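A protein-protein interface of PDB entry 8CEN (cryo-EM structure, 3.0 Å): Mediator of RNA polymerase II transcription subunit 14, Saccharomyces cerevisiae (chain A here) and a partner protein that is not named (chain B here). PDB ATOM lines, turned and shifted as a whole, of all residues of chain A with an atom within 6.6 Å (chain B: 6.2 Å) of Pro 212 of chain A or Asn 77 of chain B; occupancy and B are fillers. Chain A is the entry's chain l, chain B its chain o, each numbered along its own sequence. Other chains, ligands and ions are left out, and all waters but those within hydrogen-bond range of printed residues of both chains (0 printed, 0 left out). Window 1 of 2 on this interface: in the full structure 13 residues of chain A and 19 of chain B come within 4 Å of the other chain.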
ATOM      1  N   THR A 202      -4.346   1.875  17.343  1.00  0.00           N
ATOM      2  CA  THR A 202      -5.694   1.995  17.885  1.00  0.00           C
ATOM      3  C   THR A 202      -6.427   3.183  17.277  1.00  0.00           C
ATOM      4  O   THR A 202      -7.638   3.103  17.026  1.00  0.00           O
ATOM      5  CB  THR A 202      -5.639   2.104  19.408  1.00  0.00           C
ATOM      6  OG1 THR A 202      -4.732   1.122  19.921  1.00  0.00           O
ATOM      7  CG2 THR A 202      -7.014   1.857  20.012  1.00  0.00           C
ATOM      8  N   GLU A 205      -7.635   1.977  13.857  1.00  0.00           N
ATOM      9  CA  GLU A 205      -8.741   1.026  13.972  1.00  0.00           C
ATOM     10  C   GLU A 205     -10.046   1.735  14.317  1.00  0.00           C
ATOM     11  O   GLU A 205     -11.078   1.506  13.672  1.00  0.00           O
ATOM     12  CB  GLU A 205      -8.435  -0.052  15.014  1.00  0.00           C
ATOM     13  CG  GLU A 205      -7.268  -0.959  14.682  1.00  0.00           C
ATOM     14  CD  GLU A 205      -6.590  -1.509  15.922  1.00  0.00           C
ATOM     15  OE1 GLU A 205      -6.837  -0.977  17.022  1.00  0.00           O
ATOM     16  OE2 GLU A 205      -5.816  -2.481  15.796  1.00  0.00           O
ATOM     17  N   VAL A 206     -10.005   2.642  15.296  1.00  0.00           N
ATOM     18  CA  VAL A 206     -11.230   3.303  15.738  1.00  0.00           C
ATOM     19  C   VAL A 206     -11.731   4.290  14.689  1.00  0.00           C
ATOM     20  O   VAL A 206     -12.934   4.367  14.419  1.00  0.00           O
ATOM     21  CB  VAL A 206     -11.002   3.972  17.102  1.00  0.00           C
ATOM     22  CG1 VAL A 206     -12.231   4.737  17.532  1.00  0.00           C
ATOM     23  CG2 VAL A 206     -10.665   2.925  18.120  1.00  0.00           C
ATOM     24  N   LEU A 209     -12.871   1.651  11.338  1.00  0.00           N
ATOM     25  CA  LEU A 209     -14.000   0.740  11.469  1.00  0.00           C
ATOM     26  C   LEU A 209     -14.999   1.158  12.537  1.00  0.00           C
ATOM     27  O   LEU A 209     -16.066   0.542  12.635  1.00  0.00           O
ATOM     28  CB  LEU A 209     -13.509  -0.676  11.786  1.00  0.00           C
ATOM     29  CG  LEU A 209     -12.360  -1.260  10.969  1.00  0.00           C
ATOM     30  CD1 LEU A 209     -12.033  -2.652  11.483  1.00  0.00           C
ATOM     31  CD2 LEU A 209     -12.710  -1.297   9.492  1.00  0.00           C
ATOM     32  N   GLY A 210     -14.691   2.177  13.333  1.00  0.00           N
ATOM     33  CA  GLY A 210     -15.490   2.474  14.499  1.00  0.00           C
ATOM     34  C   GLY A 210     -15.244   1.556  15.671  1.00  0.00           C
ATOM     35  O   GLY A 210     -15.954   1.657  16.679  1.00  0.00           O
ATOM     36  N   ARG A 211     -14.258   0.671  15.573  1.00  0.00           N
ATOM     37  CA  ARG A 211     -13.982  -0.352  16.566  1.00  0.00           C
ATOM     38  C   ARG A 211     -12.487  -0.619  16.565  1.00  0.00           C
ATOM     39  O   ARG A 211     -11.842  -0.524  15.514  1.00  0.00           O
ATOM     40  CB  ARG A 211     -14.767  -1.645  16.267  1.00  0.00           C
ATOM     41  CG  ARG A 211     -14.307  -2.354  14.994  1.00  0.00           C
ATOM     42  CD  ARG A 211     -15.117  -3.565  14.583  1.00  0.00           C
ATOM     43  NE  ARG A 211     -14.449  -4.227  13.467  1.00  0.00           N
ATOM     44  CZ  ARG A 211     -14.957  -5.222  12.754  1.00  0.00           C
ATOM     45  NH1 ARG A 211     -16.163  -5.705  12.998  1.00  0.00           N
ATOM     46  NH2 ARG A 211     -14.239  -5.741  11.762  1.00  0.00           N
ATOM     47  N   PRO A 212     -11.897  -0.883  17.722  1.00  0.00           N
ATOM     48  CA  PRO A 212     -10.564  -1.486  17.739  1.00  0.00           C
ATOM     49  C   PRO A 212     -10.640  -2.936  17.294  1.00  0.00           C
ATOM     50  O   PRO A 212     -11.656  -3.613  17.471  1.00  0.00           O
ATOM     51  CB  PRO A 212     -10.131  -1.361  19.203  1.00  0.00           C
ATOM     52  CG  PRO A 212     -11.401  -1.223  19.961  1.00  0.00           C
ATOM     53  CD  PRO A 212     -12.355  -0.506  19.065  1.00  0.00           C
ATOM     54  N   ASN A 213      -9.550  -3.412  16.701  1.00  0.00           N
ATOM     55  CA  ASN A 213      -9.531  -4.743  16.101  1.00  0.00           C
ATOM     56  C   ASN A 213      -9.300  -5.776  17.196  1.00  0.00           C
ATOM     57  O   ASN A 213      -8.174  -5.976  17.656  1.00  0.00           O
ATOM     58  CB  ASN A 213      -8.460  -4.828  15.020  1.00  0.00           C
ATOM     59  CG  ASN A 213      -8.393  -6.196  14.376  1.00  0.00           C
ATOM     60  OD1 ASN A 213      -9.220  -6.538  13.530  1.00  0.00           O
ATOM     61  ND2 ASN A 213      -7.406  -6.990  14.773  1.00  0.00           N
ATOM     62  N   LEU A 214     -10.372  -6.437  17.613  1.00  0.00           N
ATOM     63  CA  LEU A 214     -10.350  -7.524  18.576  1.00  0.00           C
ATOM     64  C   LEU A 214     -10.903  -8.782  17.921  1.00  0.00           C
ATOM     65  O   LEU A 214     -11.626  -8.699  16.921  1.00  0.00           O
ATOM     66  CB  LEU A 214     -11.178  -7.182  19.825  1.00  0.00           C
ATOM     67  CG  LEU A 214     -10.587  -6.242  20.875  1.00  0.00           C
ATOM     68  CD1 LEU A 214     -10.845  -4.799  20.512  1.00  0.00           C
ATOM     69  CD2 LEU A 214     -11.144  -6.555  22.256  1.00  0.00           C
ATOM     70  N   PRO A 215     -10.546  -9.966  18.426  1.00  0.00           N
ATOM     71  CA  PRO A 215     -11.136 -11.201  17.889  1.00  0.00           C
ATOM     72  C   PRO A 215     -12.644 -11.239  18.094  1.00  0.00           C
ATOM     73  O   PRO A 215     -13.153 -10.929  19.173  1.00  0.00           O
ATOM     74  CB  PRO A 215     -10.431 -12.304  18.686  1.00  0.00           C
ATOM     75  CG  PRO A 215      -9.140 -11.703  19.100  1.00  0.00           C
ATOM     76  CD  PRO A 215      -9.410 -10.246  19.323  1.00  0.00           C
ATOM     77  N   LEU B  33     -19.088  -0.002  29.027  1.00  0.00           N
ATOM     78  CA  LEU B  33     -19.224  -1.259  28.302  1.00  0.00           C
ATOM     79  C   LEU B  33     -17.888  -1.962  28.102  1.00  0.00           C
ATOM     80  O   LEU B  33     -17.872  -3.176  27.871  1.00  0.00           O
ATOM     81  CB  LEU B  33     -19.899  -1.014  26.951  1.00  0.00           C
ATOM     82  CG  LEU B  33     -21.404  -1.290  26.867  1.00  0.00           C
ATOM     83  CD1 LEU B  33     -22.194  -0.418  27.831  1.00  0.00           C
ATOM     84  CD2 LEU B  33     -21.903  -1.089  25.449  1.00  0.00           C
ATOM     85  N   ALA B  34     -16.771  -1.231  28.173  1.00  0.00           N
ATOM     86  CA  ALA B  34     -15.462  -1.875  28.172  1.00  0.00           C
ATOM     87  C   ALA B  34     -15.281  -2.734  29.413  1.00  0.00           C
ATOM     88  O   ALA B  34     -14.684  -3.816  29.349  1.00  0.00           O
ATOM     89  CB  ALA B  34     -14.354  -0.828  28.083  1.00  0.00           C
ATOM     90  N   ILE B  73     -13.751   9.050  23.181  1.00  0.00           N
ATOM     91  CA  ILE B  73     -13.770   7.691  23.713  1.00  0.00           C
ATOM     92  C   ILE B  73     -12.367   7.350  24.202  1.00  0.00           C
ATOM     93  O   ILE B  73     -11.439   7.193  23.406  1.00  0.00           O
ATOM     94  CB  ILE B  73     -14.255   6.680  22.671  1.00  0.00           C
ATOM     95  CG1 ILE B  73     -15.677   7.021  22.222  1.00  0.00           C
ATOM     96  CG2 ILE B  73     -14.199   5.278  23.241  1.00  0.00           C
ATOM     97  CD1 ILE B  73     -16.709   6.881  23.318  1.00  0.00           C
ATOM     98  N   TYR B  75     -11.683   4.608  26.212  1.00  0.00           N
ATOM     99  CA  TYR B  75     -11.564   3.155  26.297  1.00  0.00           C
ATOM    100  C   TYR B  75     -12.270   2.510  25.107  1.00  0.00           C
ATOM    101  O   TYR B  75     -13.376   1.981  25.262  1.00  0.00           O
ATOM    102  CB  TYR B  75     -12.163   2.632  27.603  1.00  0.00           C
ATOM    103  CG  TYR B  75     -11.724   3.339  28.870  1.00  0.00           C
ATOM    104  CD1 TYR B  75     -10.494   3.065  29.448  1.00  0.00           C
ATOM    105  CD2 TYR B  75     -12.560   4.244  29.510  1.00  0.00           C
ATOM    106  CE1 TYR B  75     -10.096   3.694  30.613  1.00  0.00           C
ATOM    107  CE2 TYR B  75     -12.170   4.879  30.673  1.00  0.00           C
ATOM    108  CZ  TYR B  75     -10.937   4.599  31.220  1.00  0.00           C
ATOM    109  OH  TYR B  75     -10.544   5.227  32.378  1.00  0.00           O
ATOM    110  N   PRO B  76     -11.636   2.472  23.928  1.00  0.00           N
ATOM    111  CA  PRO B  76     -12.353   2.086  22.692  1.00  0.00           C
ATOM    112  C   PRO B  76     -12.847   0.640  22.651  1.00  0.00           C
ATOM    113  O   PRO B  76     -13.716   0.308  21.820  1.00  0.00           O
ATOM    114  CB  PRO B  76     -11.313   2.335  21.594  1.00  0.00           C
ATOM    115  CG  PRO B  76     -10.203   3.113  22.242  1.00  0.00           C
ATOM    116  CD  PRO B  76     -10.212   2.738  23.678  1.00  0.00           C
ATOM    117  N   ASN B  77     -12.352  -0.227  23.534  1.00  0.00           N
ATOM    118  CA  ASN B  77     -12.929  -1.559  23.638  1.00  0.00           C
ATOM    119  C   ASN B  77     -14.383  -1.511  24.094  1.00  0.00           C
ATOM    120  O   ASN B  77     -15.123  -2.471  23.867  1.00  0.00           O
ATOM    121  CB  ASN B  77     -12.079  -2.417  24.573  1.00  0.00           C
ATOM    122  CG  ASN B  77     -10.708  -2.707  23.992  1.00  0.00           C
ATOM    123  OD1 ASN B  77     -10.457  -2.443  22.820  1.00  0.00           O
ATOM    124  ND2 ASN B  77      -9.824  -3.262  24.799  1.00  0.00           N
ATOM    125  N   CYS B  78     -14.815  -0.393  24.686  1.00  0.00           N
ATOM    126  CA  CYS B  78     -16.236  -0.177  24.930  1.00  0.00           C
ATOM    127  C   CYS B  78     -17.008  -0.081  23.623  1.00  0.00           C
ATOM    128  O   CYS B  78     -18.120  -0.605  23.516  1.00  0.00           O
ATOM    129  CB  CYS B  78     -16.451   1.101  25.724  1.00  0.00           C
ATOM    130  SG  CYS B  78     -16.345   2.627  24.747  1.00  0.00           S
ATOM    131  N   LEU B  79     -16.450   0.621  22.630  1.00  0.00           N
ATOM    132  CA  LEU B  79     -17.075   0.671  21.311  1.00  0.00           C
ATOM    133  C   LEU B  79     -17.110  -0.711  20.676  1.00  0.00           C
ATOM    134  O   LEU B  79     -18.094  -1.078  20.017  1.00  0.00           O
ATOM    135  CB  LEU B  79     -16.330   1.647  20.401  1.00  0.00           C
ATOM    136  CG  LEU B  79     -16.434   3.139  20.696  1.00  0.00           C
ATOM    137  CD1 LEU B  79     -15.335   3.890  19.968  1.00  0.00           C
ATOM    138  CD2 LEU B  79     -17.796   3.649  20.282  1.00  0.00           C
ATOM    139  N   PHE B  80     -16.036  -1.483  20.863  1.00  0.00           N
ATOM    140  CA  PHE B  80     -16.028  -2.867  20.381  1.00  0.00           C
ATOM    141  C   PHE B  80     -17.155  -3.687  21.011  1.00  0.00           C
ATOM    142  O   PHE B  80     -17.892  -4.395  20.311  1.00  0.00           O
ATOM    143  CB  PHE B  80     -14.682  -3.533  20.664  1.00  0.00           C
ATOM    144  CG  PHE B  80     -14.663  -4.999  20.330  1.00  0.00           C
ATOM    145  CD1 PHE B  80     -14.675  -5.423  19.011  1.00  0.00           C
ATOM    146  CD2 PHE B  80     -14.666  -5.954  21.336  1.00  0.00           C
ATOM    147  CE1 PHE B  80     -14.671  -6.771  18.704  1.00  0.00           C
ATOM    148  CE2 PHE B  80     -14.667  -7.301  21.033  1.00  0.00           C
ATOM    149  CZ  PHE B  80     -14.672  -7.710  19.715  1.00  0.00           C
ATOM    150  N   ILE B  81     -17.307  -3.588  22.334  1.00  0.00           N
ATOM    151  CA  ILE B  81     -18.365  -4.307  23.040  1.00  0.00           C
ATOM    152  C   ILE B  81     -19.742  -3.798  22.618  1.00  0.00           C
ATOM    153  O   ILE B  81     -20.694  -4.579  22.530  1.00  0.00           O
ATOM    154  CB  ILE B  81     -18.139  -4.200  24.564  1.00  0.00           C
ATOM    155  CG1 ILE B  81     -16.876  -4.965  24.965  1.00  0.00           C
ATOM    156  CG2 ILE B  81     -19.319  -4.748  25.357  1.00  0.00           C
ATOM    157  CD1 ILE B  81     -16.936  -6.449  24.670  1.00  0.00           C
ATOM    158  N   LEU B  82     -19.865  -2.501  22.330  1.00  0.00           N
ATOM    159  CA  LEU B  82     -21.138  -1.943  21.879  1.00  0.00           C
ATOM    160  C   LEU B  82     -21.557  -2.528  20.536  1.00  0.00           C
ATOM    161  O   LEU B  82     -22.718  -2.913  20.351  1.00  0.00           O
ATOM    162  CB  LEU B  82     -21.040  -0.421  21.789  1.00  0.00           C
ATOM    163  CG  LEU B  82     -22.177   0.253  21.018  1.00  0.00           C
ATOM    164  CD1 LEU B  82     -23.427   0.345  21.879  1.00  0.00           C
ATOM    165  CD2 LEU B  82     -21.759   1.619  20.501  1.00  0.00           C
ATOM    166  N   MET B 121      -8.458  -8.737  25.515  1.00  0.00           N
ATOM    167  CA  MET B 121      -8.162  -7.307  25.493  1.00  0.00           C
ATOM    168  C   MET B 121      -7.006  -6.933  26.420  1.00  0.00           C
ATOM    169  O   MET B 121      -6.309  -5.952  26.148  1.00  0.00           O
ATOM    170  CB  MET B 121      -9.417  -6.487  25.815  1.00  0.00           C
ATOM    171  CG  MET B 121      -9.986  -6.662  27.195  1.00  0.00           C
ATOM    172  SD  MET B 121     -11.521  -5.738  27.431  1.00  0.00           S
ATOM    173  CE  MET B 121     -12.674  -6.710  26.470  1.00  0.00           C
ATOM    174  N   VAL B 122      -6.744  -7.719  27.468  1.00  0.00           N
ATOM    175  CA  VAL B 122      -5.521  -7.529  28.246  1.00  0.00           C
ATOM    176  C   VAL B 122      -4.293  -7.918  27.422  1.00  0.00           C
ATOM    177  O   VAL B 122      -3.237  -7.278  27.510  1.00  0.00           O
ATOM    178  CB  VAL B 122      -5.619  -8.306  29.575  1.00  0.00           C
ATOM    179  CG1 VAL B 122      -4.257  -8.518  30.219  1.00  0.00           C
ATOM    180  CG2 VAL B 122      -6.518  -7.556  30.542  1.00  0.00           C
ATOM    181  N   ARG B 124      -4.176  -7.573  24.160  1.00  0.00           N
ATOM    182  CA  ARG B 124      -4.028  -6.417  23.277  1.00  0.00           C
ATOM    183  C   ARG B 124      -3.398  -5.232  23.997  1.00  0.00           C
ATOM    184  O   ARG B 124      -2.679  -4.441  23.376  1.00  0.00           O
ATOM    185  CB  ARG B 124      -5.374  -6.005  22.688  1.00  0.00           C
ATOM    186  CG  ARG B 124      -5.788  -6.794  21.468  1.00  0.00           C
ATOM    187  CD  ARG B 124      -6.903  -6.082  20.726  1.00  0.00           C
ATOM    188  NE  ARG B 124      -6.397  -5.111  19.763  1.00  0.00           N
ATOM    189  CZ  ARG B 124      -6.300  -3.808  19.990  1.00  0.00           C
ATOM    190  NH1 ARG B 124      -6.668  -3.277  21.144  1.00  0.00           N
ATOM    191  NH2 ARG B 124      -5.823  -3.017  19.033  1.00  0.00           N
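The guanidinium group (NH2) of Arg 124 of chain B lies within salt-bridge range of the side-chain carboxylate (OE1) of Glu 205 of chain A. O of Asn 213 of chain A lies within hydrogen-bond range of NE of Arg 124 of chain B (2.9 Å).
Among the printed residues, pairs that only touch across the chains: Val 206 of chain A with Pro 76 of chain B (3.6 Å), Gly 210 of chain A with Leu 79 of chain B (3.7 Å), Pro 212 of chain A with Pro 76 of chain B (3.2 Å), Pro 212 of chain A with Asn 77 of chain B (3.2 Å), Pro 212 of chain A with Phe 80 of chain B (3.8 Å), Leu 214 of chain A with Asn 77 of chain B (3.3 Å), Leu 214 of chain A with Phe 80 of chain B (3.5 Å), Leu 214 of chain A with Met 121 of chain B (3.96 Å), Leu 214 of chain A with Arg 124 of chain B (3.7 Å) and Pro 215 of chain A with Phe 80 of chain B (3.6 Å).
Of the printed residues of chain B, Glu 205 of chain A touches Arg 124 (3.0 Å). Pro 212 of chain A touches just these residues of chain B: Pro 76 (3.2 Å), Asn 77 (3.2 Å) and Phe 80 (3.8 Å). Printed residues of chain B within 4 Å of Asn 213 of chain A: Arg 124 (2.9 Å). Ile 73 of chain B touches none of the printed residues of chain A. Asn 77 of chain B touches just these residues of chain A: Pro 212 (3.2 Å) and Leu 214 (3.3 Å). Printed residues of chain A within 4 Å of Leu 79 of chain B: Gly 210. Of the printed residues of chain A, Phe 80 of chain B touches Pro 212, Leu 214 and Pro 215. Of the printed residues of chain A, Arg 124 of chain B touches Glu 205 (3.0 Å), Asn 213 (2.9 Å) and Leu 214 (3.7 Å). The nearest residue of chain B that does not touch Pro 212 of chain A is Arg 124 of chain B (4.4 Å). The nearest residue of chain A that does not touch Asn 77 of chain B is Thr 202 of chain A (6.2 Å).
Printed residues of chain A that touch a printed residue of chain B: Glu 205, Val 206, Gly 210, Pro 212, Asn 213, Leu 214 and Pro 215. Of the 14 printed residues of chain B, 6 touch a printed residue of chain A. Hydrophobic or aromatic side chains of chain B that line the printed part of chain A: Pro 76, Leu 79, Phe 80 and Met 121. Among the printed residues, Asp or Glu carboxylates within 4 Å of a Lys or Arg side-chain nitrogen of the other chain: Glu 205 of chain A with Arg 124 of chain B (3.0 Å).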
